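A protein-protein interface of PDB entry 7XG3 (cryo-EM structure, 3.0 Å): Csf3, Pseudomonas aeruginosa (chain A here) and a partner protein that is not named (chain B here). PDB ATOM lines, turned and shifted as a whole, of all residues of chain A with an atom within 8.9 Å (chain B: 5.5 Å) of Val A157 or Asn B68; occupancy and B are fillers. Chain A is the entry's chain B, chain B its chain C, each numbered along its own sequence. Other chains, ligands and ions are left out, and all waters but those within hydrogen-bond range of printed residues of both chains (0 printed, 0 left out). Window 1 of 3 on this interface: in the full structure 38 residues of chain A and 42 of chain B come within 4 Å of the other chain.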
ATOM      1  N   ASN A  12      -9.700   9.594   4.266  1.00  0.00           N
ATOM      2  CA  ASN A  12     -11.134   9.551   4.045  1.00  0.00           C
ATOM      3  C   ASN A  12     -11.501  10.598   3.008  1.00  0.00           C
ATOM      4  O   ASN A  12     -10.853  11.646   2.929  1.00  0.00           O
ATOM      5  CB  ASN A  12     -11.904   9.839   5.341  1.00  0.00           C
ATOM      6  CG  ASN A  12     -12.896   8.755   5.690  1.00  0.00           C
ATOM      7  OD1 ASN A  12     -13.118   7.825   4.919  1.00  0.00           O
ATOM      8  ND2 ASN A  12     -13.500   8.869   6.864  1.00  0.00           N
ATOM      9  N   PRO A  13     -12.520  10.341   2.191  1.00  0.00           N
ATOM     10  CA  PRO A  13     -12.997  11.374   1.267  1.00  0.00           C
ATOM     11  C   PRO A  13     -13.625  12.549   2.005  1.00  0.00           C
ATOM     12  O   PRO A  13     -14.173  12.403   3.098  1.00  0.00           O
ATOM     13  CB  PRO A  13     -14.027  10.631   0.414  1.00  0.00           C
ATOM     14  CG  PRO A  13     -13.634   9.212   0.497  1.00  0.00           C
ATOM     15  CD  PRO A  13     -13.109   9.027   1.885  1.00  0.00           C
ATOM     16  N   MET A  15     -15.683  16.613   1.834  1.00  0.00           N
ATOM     17  CA  MET A  15     -16.620  17.483   1.135  1.00  0.00           C
ATOM     18  C   MET A  15     -15.869  18.400   0.180  1.00  0.00           C
ATOM     19  O   MET A  15     -14.889  19.043   0.566  1.00  0.00           O
ATOM     20  CB  MET A  15     -17.413  18.324   2.136  1.00  0.00           C
ATOM     21  CG  MET A  15     -18.222  17.542   3.157  1.00  0.00           C
ATOM     22  SD  MET A  15     -19.147  16.179   2.449  1.00  0.00           S
ATOM     23  CE  MET A  15     -20.518  16.040   3.587  1.00  0.00           C
ATOM     24  N   TRP A  82     -22.381  12.464  -1.961  1.00  0.00           N
ATOM     25  CA  TRP A  82     -22.864  11.916  -0.708  1.00  0.00           C
ATOM     26  C   TRP A  82     -24.279  12.401  -0.476  1.00  0.00           C
ATOM     27  O   TRP A  82     -24.603  13.558  -0.758  1.00  0.00           O
ATOM     28  CB  TRP A  82     -21.992  12.326   0.474  1.00  0.00           C
ATOM     29  CG  TRP A  82     -22.217  11.486   1.676  1.00  0.00           C
ATOM     30  CD1 TRP A  82     -22.742  11.887   2.864  1.00  0.00           C
ATOM     31  CD2 TRP A  82     -21.928  10.092   1.813  1.00  0.00           C
ATOM     32  NE1 TRP A  82     -22.802  10.829   3.737  1.00  0.00           N
ATOM     33  CE2 TRP A  82     -22.314   9.714   3.112  1.00  0.00           C
ATOM     34  CE3 TRP A  82     -21.382   9.127   0.963  1.00  0.00           C
ATOM     35  CZ2 TRP A  82     -22.159   8.418   3.584  1.00  0.00           C
ATOM     36  CZ3 TRP A  82     -21.241   7.841   1.429  1.00  0.00           C
ATOM     37  CH2 TRP A  82     -21.628   7.497   2.727  1.00  0.00           C
ATOM     38  N   MET A  83     -25.113  11.511   0.033  1.00  0.00           N
ATOM     39  CA  MET A  83     -26.475  11.828   0.416  1.00  0.00           C
ATOM     40  C   MET A  83     -26.583  11.681   1.922  1.00  0.00           C
ATOM     41  O   MET A  83     -26.014  10.750   2.501  1.00  0.00           O
ATOM     42  CB  MET A  83     -27.447  10.907  -0.325  1.00  0.00           C
ATOM     43  CG  MET A  83     -28.926  10.897   0.072  1.00  0.00           C
ATOM     44  SD  MET A  83     -29.398  10.006   1.568  1.00  0.00           S
ATOM     45  CE  MET A  83     -29.972   8.520   0.816  1.00  0.00           C
ATOM     46  N   GLN A  84     -27.331  12.582   2.548  1.00  0.00           N
ATOM     47  CA  GLN A  84     -27.675  12.446   3.951  1.00  0.00           C
ATOM     48  C   GLN A  84     -29.131  12.841   4.140  1.00  0.00           C
ATOM     49  O   GLN A  84     -29.681  13.641   3.376  1.00  0.00           O
ATOM     50  CB  GLN A  84     -26.764  13.293   4.841  1.00  0.00           C
ATOM     51  CG  GLN A  84     -25.382  12.719   5.034  1.00  0.00           C
ATOM     52  CD  GLN A  84     -24.355  13.754   5.438  1.00  0.00           C
ATOM     53  OE1 GLN A  84     -24.444  14.916   5.053  1.00  0.00           O
ATOM     54  NE2 GLN A  84     -23.372  13.334   6.221  1.00  0.00           N
ATOM     55  N   THR A  85     -29.758  12.252   5.154  1.00  0.00           N
ATOM     56  CA  THR A  85     -31.153  12.519   5.464  1.00  0.00           C
ATOM     57  C   THR A  85     -31.305  12.842   6.939  1.00  0.00           C
ATOM     58  O   THR A  85     -30.466  12.486   7.768  1.00  0.00           O
ATOM     59  CB  THR A  85     -32.073  11.340   5.124  1.00  0.00           C
ATOM     60  OG1 THR A  85     -31.568  10.141   5.722  1.00  0.00           O
ATOM     61  CG2 THR A  85     -32.195  11.165   3.627  1.00  0.00           C
ATOM     62  N   GLY A  86     -32.386  13.543   7.243  1.00  0.00           N
ATOM     63  CA  GLY A  86     -32.710  13.906   8.603  1.00  0.00           C
ATOM     64  C   GLY A  86     -34.181  13.735   8.896  1.00  0.00           C
ATOM     65  O   GLY A  86     -35.022  14.289   8.186  1.00  0.00           O
ATOM     66  N   ARG A  87     -34.504  12.961   9.929  1.00  0.00           N
ATOM     67  CA  ARG A  87     -35.884  12.788  10.354  1.00  0.00           C
ATOM     68  C   ARG A  87     -35.909  12.373  11.816  1.00  0.00           C
ATOM     69  O   ARG A  87     -35.045  11.622  12.274  1.00  0.00           O
ATOM     70  CB  ARG A  87     -36.617  11.746   9.500  1.00  0.00           C
ATOM     71  CG  ARG A  87     -35.881  10.438   9.373  1.00  0.00           C
ATOM     72  CD  ARG A  87     -36.700   9.368   8.688  1.00  0.00           C
ATOM     73  NE  ARG A  87     -35.864   8.193   8.507  1.00  0.00           N
ATOM     74  CZ  ARG A  87     -35.011   8.040   7.505  1.00  0.00           C
ATOM     75  NH1 ARG A  87     -34.967   8.895   6.496  1.00  0.00           N
ATOM     76  NH2 ARG A  87     -34.153   7.025   7.533  1.00  0.00           N
ATOM     77  N   TYR A 121     -30.407  15.645   1.346  1.00  0.00           N
ATOM     78  CA  TYR A 121     -29.482  16.640   0.820  1.00  0.00           C
ATOM     79  C   TYR A 121     -28.201  15.964   0.363  1.00  0.00           C
ATOM     80  O   TYR A 121     -27.721  15.017   0.993  1.00  0.00           O
ATOM     81  CB  TYR A 121     -29.168  17.749   1.846  1.00  0.00           C
ATOM     82  CG  TYR A 121     -28.614  17.300   3.181  1.00  0.00           C
ATOM     83  CD1 TYR A 121     -29.438  16.757   4.161  1.00  0.00           C
ATOM     84  CD2 TYR A 121     -27.270  17.463   3.476  1.00  0.00           C
ATOM     85  CE1 TYR A 121     -28.930  16.353   5.374  1.00  0.00           C
ATOM     86  CE2 TYR A 121     -26.757  17.076   4.695  1.00  0.00           C
ATOM     87  CZ  TYR A 121     -27.593  16.530   5.640  1.00  0.00           C
ATOM     88  OH  TYR A 121     -27.087  16.129   6.853  1.00  0.00           O
ATOM     89  N   ILE A 125     -18.348  14.931  -3.083  1.00  0.00           N
ATOM     90  CA  ILE A 125     -17.336  14.191  -2.340  1.00  0.00           C
ATOM     91  C   ILE A 125     -16.124  14.032  -3.244  1.00  0.00           C
ATOM     92  O   ILE A 125     -16.246  13.552  -4.379  1.00  0.00           O
ATOM     93  CB  ILE A 125     -17.867  12.821  -1.874  1.00  0.00           C
ATOM     94  CG1 ILE A 125     -18.616  12.955  -0.563  1.00  0.00           C
ATOM     95  CG2 ILE A 125     -16.755  11.843  -1.624  1.00  0.00           C
ATOM     96  CD1 ILE A 125     -17.781  13.485   0.553  1.00  0.00           C
ATOM     97  N   GLN A 150      -9.186  16.354  10.652  1.00  0.00           N
ATOM     98  CA  GLN A 150     -10.116  16.459   9.537  1.00  0.00           C
ATOM     99  C   GLN A 150      -9.911  17.789   8.822  1.00  0.00           C
ATOM    100  O   GLN A 150      -9.369  18.733   9.398  1.00  0.00           O
ATOM    101  CB  GLN A 150     -11.568  16.308  10.006  1.00  0.00           C
ATOM    102  CG  GLN A 150     -12.012  14.855  10.089  1.00  0.00           C
ATOM    103  CD  GLN A 150     -12.917  14.567  11.265  1.00  0.00           C
ATOM    104  OE1 GLN A 150     -12.578  14.847  12.414  1.00  0.00           O
ATOM    105  NE2 GLN A 150     -14.079  13.996  10.982  1.00  0.00           N
ATOM    106  N   GLY A 153     -14.429  19.540   5.946  1.00  0.00           N
ATOM    107  CA  GLY A 153     -15.567  19.487   6.826  1.00  0.00           C
ATOM    108  C   GLY A 153     -15.146  18.945   8.173  1.00  0.00           C
ATOM    109  O   GLY A 153     -14.613  17.836   8.258  1.00  0.00           O
ATOM    110  N   LYS A 154     -15.380  19.711   9.239  1.00  0.00           N
ATOM    111  CA  LYS A 154     -15.250  19.207  10.608  1.00  0.00           C
ATOM    112  C   LYS A 154     -16.577  18.576  11.037  1.00  0.00           C
ATOM    113  O   LYS A 154     -17.165  18.912  12.064  1.00  0.00           O
ATOM    114  CB  LYS A 154     -14.840  20.330  11.550  1.00  0.00           C
ATOM    115  CG  LYS A 154     -14.156  19.871  12.829  1.00  0.00           C
ATOM    116  CD  LYS A 154     -14.193  20.955  13.893  1.00  0.00           C
ATOM    117  CE  LYS A 154     -13.603  20.459  15.206  1.00  0.00           C
ATOM    118  NZ  LYS A 154     -13.465  21.548  16.213  1.00  0.00           N
ATOM    119  N   ARG A 155     -17.031  17.626  10.214  1.00  0.00           N
ATOM    120  CA  ARG A 155     -18.422  17.200  10.197  1.00  0.00           C
ATOM    121  C   ARG A 155     -18.824  16.445  11.447  1.00  0.00           C
ATOM    122  O   ARG A 155     -20.014  16.408  11.777  1.00  0.00           O
ATOM    123  CB  ARG A 155     -18.677  16.342   8.961  1.00  0.00           C
ATOM    124  CG  ARG A 155     -18.576  17.064   7.632  1.00  0.00           C
ATOM    125  CD  ARG A 155     -19.942  17.554   7.193  1.00  0.00           C
ATOM    126  NE  ARG A 155     -19.866  18.464   6.058  1.00  0.00           N
ATOM    127  CZ  ARG A 155     -20.914  19.059   5.504  1.00  0.00           C
ATOM    128  NH1 ARG A 155     -22.143  18.851   5.948  1.00  0.00           N
ATOM    129  NH2 ARG A 155     -20.724  19.890   4.482  1.00  0.00           N
ATOM    130  N   GLY A 156     -17.864  15.858  12.153  1.00  0.00           N
ATOM    131  CA  GLY A 156     -18.178  14.975  13.243  1.00  0.00           C
ATOM    132  C   GLY A 156     -18.917  13.727  12.837  1.00  0.00           C
ATOM    133  O   GLY A 156     -19.566  13.106  13.688  1.00  0.00           O
ATOM    134  N   VAL A 157     -18.870  13.350  11.563  1.00  0.00           N
ATOM    135  CA  VAL A 157     -19.680  12.249  11.079  1.00  0.00           C
ATOM    136  C   VAL A 157     -18.751  11.349  10.272  1.00  0.00           C
ATOM    137  O   VAL A 157     -19.124  10.238   9.880  1.00  0.00           O
ATOM    138  CB  VAL A 157     -20.877  12.771  10.263  1.00  0.00           C
ATOM    139  CG1 VAL A 157     -20.467  13.226   8.895  1.00  0.00           C
ATOM    140  CG2 VAL A 157     -21.979  11.798  10.219  1.00  0.00           C
ATOM    141  N   GLY A 158     -17.527  11.820  10.034  1.00  0.00           N
ATOM    142  CA  GLY A 158     -16.459  10.962   9.566  1.00  0.00           C
ATOM    143  C   GLY A 158     -15.736  11.356   8.295  1.00  0.00           C
ATOM    144  O   GLY A 158     -14.982  10.533   7.765  1.00  0.00           O
ATOM    145  N   PHE A 159     -15.918  12.572   7.795  1.00  0.00           N
ATOM    146  CA  PHE A 159     -15.371  12.915   6.488  1.00  0.00           C
ATOM    147  C   PHE A 159     -14.128  13.783   6.579  1.00  0.00           C
ATOM    148  O   PHE A 159     -13.977  14.606   7.484  1.00  0.00           O
ATOM    149  CB  PHE A 159     -16.411  13.614   5.612  1.00  0.00           C
ATOM    150  CG  PHE A 159     -17.515  12.716   5.170  1.00  0.00           C
ATOM    151  CD1 PHE A 159     -18.578  12.434   6.004  1.00  0.00           C
ATOM    152  CD2 PHE A 159     -17.465  12.119   3.924  1.00  0.00           C
ATOM    153  CE1 PHE A 159     -19.579  11.595   5.604  1.00  0.00           C
ATOM    154  CE2 PHE A 159     -18.465  11.278   3.515  1.00  0.00           C
ATOM    155  CZ  PHE A 159     -19.521  11.015   4.361  1.00  0.00           C
ATOM    156  N   GLY A 160     -13.244  13.597   5.604  1.00  0.00           N
ATOM    157  CA  GLY A 160     -12.052  14.407   5.483  1.00  0.00           C
ATOM    158  C   GLY A 160     -10.923  14.041   6.414  1.00  0.00           C
ATOM    159  O   GLY A 160     -10.085  14.895   6.706  1.00  0.00           O
ATOM    160  N   GLN A 161     -10.861  12.787   6.865  1.00  0.00           N
ATOM    161  CA  GLN A 161      -9.842  12.376   7.826  1.00  0.00           C
ATOM    162  C   GLN A 161      -8.454  12.398   7.200  1.00  0.00           C
ATOM    163  O   GLN A 161      -8.226  11.836   6.125  1.00  0.00           O
ATOM    164  CB  GLN A 161     -10.159  10.986   8.369  1.00  0.00           C
ATOM    165  CG  GLN A 161     -11.232  10.988   9.435  1.00  0.00           C
ATOM    166  CD  GLN A 161     -11.857   9.627   9.635  1.00  0.00           C
ATOM    167  OE1 GLN A 161     -11.298   8.606   9.238  1.00  0.00           O
ATOM    168  NE2 GLN A 161     -13.030   9.605  10.250  1.00  0.00           N
ATOM    169  N   PRO B  66     -23.497   4.644   6.599  1.00  0.00           N
ATOM    170  CA  PRO B  66     -23.088   6.045   6.740  1.00  0.00           C
ATOM    171  C   PRO B  66     -22.910   6.431   8.197  1.00  0.00           C
ATOM    172  O   PRO B  66     -23.480   5.817   9.102  1.00  0.00           O
ATOM    173  CB  PRO B  66     -24.246   6.822   6.108  1.00  0.00           C
ATOM    174  CG  PRO B  66     -24.915   5.864   5.237  1.00  0.00           C
ATOM    175  CD  PRO B  66     -24.757   4.517   5.853  1.00  0.00           C
ATOM    176  N   GLY B  67     -22.082   7.453   8.415  1.00  0.00           N
ATOM    177  CA  GLY B  67     -21.787   7.873   9.773  1.00  0.00           C
ATOM    178  C   GLY B  67     -22.968   8.531  10.455  1.00  0.00           C
ATOM    179  O   GLY B  67     -23.029   8.587  11.684  1.00  0.00           O
ATOM    180  N   ASN B  68     -23.894   9.084   9.666  1.00  0.00           N
ATOM    181  CA  ASN B  68     -25.091   9.696  10.233  1.00  0.00           C
ATOM    182  C   ASN B  68     -25.980   8.657  10.891  1.00  0.00           C
ATOM    183  O   ASN B  68     -26.577   8.915  11.943  1.00  0.00           O
ATOM    184  CB  ASN B  68     -25.860  10.445   9.150  1.00  0.00           C
ATOM    185  CG  ASN B  68     -25.268  11.794   8.854  1.00  0.00           C
ATOM    186  OD1 ASN B  68     -24.405  11.922   7.995  1.00  0.00           O
ATOM    187  ND2 ASN B  68     -25.734  12.814   9.558  1.00  0.00           N
ATOM    188  N   THR B  69     -26.080   7.475  10.277  1.00  0.00           N
ATOM    189  CA  THR B  69     -26.813   6.368  10.880  1.00  0.00           C
ATOM    190  C   THR B  69     -26.153   5.933  12.182  1.00  0.00           C
ATOM    191  O   THR B  69     -26.836   5.647  13.170  1.00  0.00           O
ATOM    192  CB  THR B  69     -26.895   5.205   9.892  1.00  0.00           C
ATOM    193  OG1 THR B  69     -27.505   5.657   8.678  1.00  0.00           O
ATOM    194  CG2 THR B  69     -27.725   4.064  10.463  1.00  0.00           C
ATOM    195  N   MET B  70     -24.816   5.931  12.209  1.00  0.00           N
ATOM    196  CA  MET B  70     -24.078   5.611  13.428  1.00  0.00           C
ATOM    197  C   MET B  70     -24.336   6.636  14.521  1.00  0.00           C
ATOM    198  O   MET B  70     -24.550   6.275  15.686  1.00  0.00           O
ATOM    199  CB  MET B  70     -22.580   5.576  13.135  1.00  0.00           C
ATOM    200  CG  MET B  70     -22.114   4.598  12.106  1.00  0.00           C
ATOM    201  SD  MET B  70     -23.026   3.086  12.160  1.00  0.00           S
ATOM    202  CE  MET B  70     -22.456   2.305  13.671  1.00  0.00           C
ATOM    203  N   ARG B  71     -24.317   7.916  14.146  1.00  0.00           N
ATOM    204  CA  ARG B  71     -24.498   9.008  15.094  1.00  0.00           C
ATOM    205  C   ARG B  71     -25.901   8.987  15.676  1.00  0.00           C
ATOM    206  O   ARG B  71     -26.083   9.101  16.894  1.00  0.00           O
ATOM    207  CB  ARG B  71     -24.213  10.334  14.386  1.00  0.00           C
ATOM    208  CG  ARG B  71     -23.969  11.531  15.282  1.00  0.00           C
ATOM    209  CD  ARG B  71     -23.433  12.680  14.442  1.00  0.00           C
ATOM    210  NE  ARG B  71     -23.320  13.931  15.181  1.00  0.00           N
ATOM    211  CZ  ARG B  71     -22.177  14.445  15.614  1.00  0.00           C
ATOM    212  NH1 ARG B  71     -21.023  13.833  15.408  1.00  0.00           N
ATOM    213  NH2 ARG B  71     -22.192  15.604  16.264  1.00  0.00           N
ATOM    214  N   SER B  72     -26.903   8.783  14.818  1.00  0.00           N
ATOM    215  CA  SER B  72     -28.281   8.719  15.286  1.00  0.00           C
ATOM    216  C   SER B  72     -28.540   7.450  16.084  1.00  0.00           C
ATOM    217  O   SER B  72     -29.347   7.462  17.013  1.00  0.00           O
ATOM    218  CB  SER B  72     -29.245   8.813  14.110  1.00  0.00           C
ATOM    219  OG  SER B  72     -30.577   8.570  14.526  1.00  0.00           O
ATOM    220  N   LEU B  73     -27.855   6.352  15.755  1.00  0.00           N
ATOM    221  CA  LEU B  73     -28.026   5.116  16.513  1.00  0.00           C
ATOM    222  C   LEU B  73     -27.456   5.251  17.918  1.00  0.00           C
ATOM    223  O   LEU B  73     -28.089   4.839  18.899  1.00  0.00           O
ATOM    224  CB  LEU B  73     -27.363   3.958  15.771  1.00  0.00           C
ATOM    225  CG  LEU B  73     -27.365   2.617  16.499  1.00  0.00           C
ATOM    226  CD1 LEU B  73     -28.786   2.141  16.736  1.00  0.00           C
ATOM    227  CD2 LEU B  73     -26.576   1.594  15.708  1.00  0.00           C
ATOM    228  N   MET B 145     -17.446  13.051  17.305  1.00  0.00           N
ATOM    229  CA  MET B 145     -17.233  12.803  15.860  1.00  0.00           C
ATOM    230  C   MET B 145     -17.495  11.307  15.689  1.00  0.00           C
ATOM    231  O   MET B 145     -16.663  10.507  16.157  1.00  0.00           O
ATOM    232  CB  MET B 145     -15.794  13.120  15.443  1.00  0.00           C
ATOM    233  CG  MET B 145     -15.564  13.046  13.945  1.00  0.00           C
ATOM    234  SD  MET B 145     -15.842  11.392  13.259  1.00  0.00           S
ATOM    235  CE  MET B 145     -14.502  10.483  14.028  1.00  0.00           C
ATOM    236  N   VAL B 146     -18.618  10.951  15.067  1.00  0.00           N
ATOM    237  CA  VAL B 146     -18.961   9.510  14.899  1.00  0.00           C
ATOM    238  C   VAL B 146     -18.623   9.132  13.462  1.00  0.00           C
ATOM    239  O   VAL B 146     -19.141   9.792  12.543  1.00  0.00           O
ATOM    240  CB  VAL B 146     -20.441   9.234  15.221  1.00  0.00           C
ATOM    241  CG1 VAL B 146     -20.904   7.910  14.632  1.00  0.00           C
ATOM    242  CG2 VAL B 146     -20.711   9.281  16.717  1.00  0.00           C
ATOM    243  N   ASP B 147     -17.784   8.112  13.287  1.00  0.00           N
ATOM    244  CA  ASP B 147     -17.414   7.731  11.933  1.00  0.00           C
ATOM    245  C   ASP B 147     -18.392   6.702  11.384  1.00  0.00           C
ATOM    246  O   ASP B 147     -19.234   6.160  12.102  1.00  0.00           O
ATOM    247  CB  ASP B 147     -15.984   7.179  11.902  1.00  0.00           C
ATOM    248  CG  ASP B 147     -15.305   7.374  10.557  1.00  0.00           C
ATOM    249  OD1 ASP B 147     -16.006   7.681   9.571  1.00  0.00           O
ATOM    250  OD2 ASP B 147     -14.067   7.224  10.489  1.00  0.00           O
ATOM    251  N   SER B 148     -18.273   6.460  10.080  1.00  0.00           N
ATOM    252  CA  SER B 148     -19.041   5.428   9.408  1.00  0.00           C
ATOM    253  C   SER B 148     -18.665   4.055   9.945  1.00  0.00           C
ATOM    254  O   SER B 148     -17.552   3.842  10.432  1.00  0.00           O
ATOM    255  CB  SER B 148     -18.783   5.494   7.903  1.00  0.00           C
ATOM    256  OG  SER B 148     -19.118   6.766   7.381  1.00  0.00           O
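Of the printed residues of chain B, Val A157 touches Gly B67 (3.4 Å), Asn B68 (3.3 Å), Met B145 (3.98 Å), Val B146 (2.7 Å), Asp B147 (3.7 Å) and Ser B148 (3.9 Å).
Asn B68 touches two residues of chain A.
Printed residues of chain A within 4 Å of Pro B66: Trp A82 (3.6 Å).
Of the printed residues of chain B, Gly A156 touches Arg B71 (2.4 Å), Met B145 (3.2 Å) and Val B146 (2.7 Å).
Printed residues of chain B within 4 Å of Trp A82: Pro B66.
Printed residues of chain A within 4 Å of Met B145: Gln A150, Gly A156, Val A157 and Gly A158.
NE2 of Gln A161 sits at hydrogen-bond distance from O of Gly A158, 3.3 Å away.
OG of Ser B148 is in hydrogen-bond range of N of Gly B67 (3.2 Å).
ND2 of Asn A12 sits at hydrogen-bond distance from O of Gly A158, 2.4 Å away.
OE1 of Gln A161 lies within hydrogen-bond range of ND2 of Asn A12 (3.2 Å).
N of Gln A84 sits at hydrogen-bond distance from O of Tyr A121 (2.9 Å).
Among the printed residues, pairs that only touch across the chains: Gly A156 with Met B145, Val A157 with Asn B68, Gly A158 with Asp B147, Val A157 with Gly B67, Gln A150 with Met B145, Gly A158 with Val B146, Trp A82 with Pro B66, Val A157 with Asp B147, Asn A12 with Asp B147, Val A157 with Ser B148 and Val A157 with Met B145.
Hydrophobic or aromatic side chains of chain B that line the printed part of chain A: Pro B66 and Met B145.
Of the 21 printed residues of chain A, 8 touch a printed residue of chain B.
Hydrophobic or aromatic side chains of chain A that line the printed part of chain B: Trp A82 and Val A157.
Among the printed residues, no Asp or Glu carboxylate lies within 4 Å of a Lys or Arg side-chain nitrogen of the other chain.
NH1 of Arg B71 lies close to O of Gly A156 (2.4 Å).
NE2 of Gln A84 lies within hydrogen-bond range of OD1 of Asn B68 (2.5 Å).
The backbone carbonyl oxygen (O) of Gly A156 sits at hydrogen-bond distance from the backbone NH (N) of Val B146 (2.7 Å).
N of Gly A158 is in hydrogen-bond range of SD of Met B145 (3.7 Å).
O of Val A157 sits close to O of Val B146 (2.7 Å).
NE2 of Gln A161 is in hydrogen-bond range of OD2 of Asp B147, at 2.6 Å.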
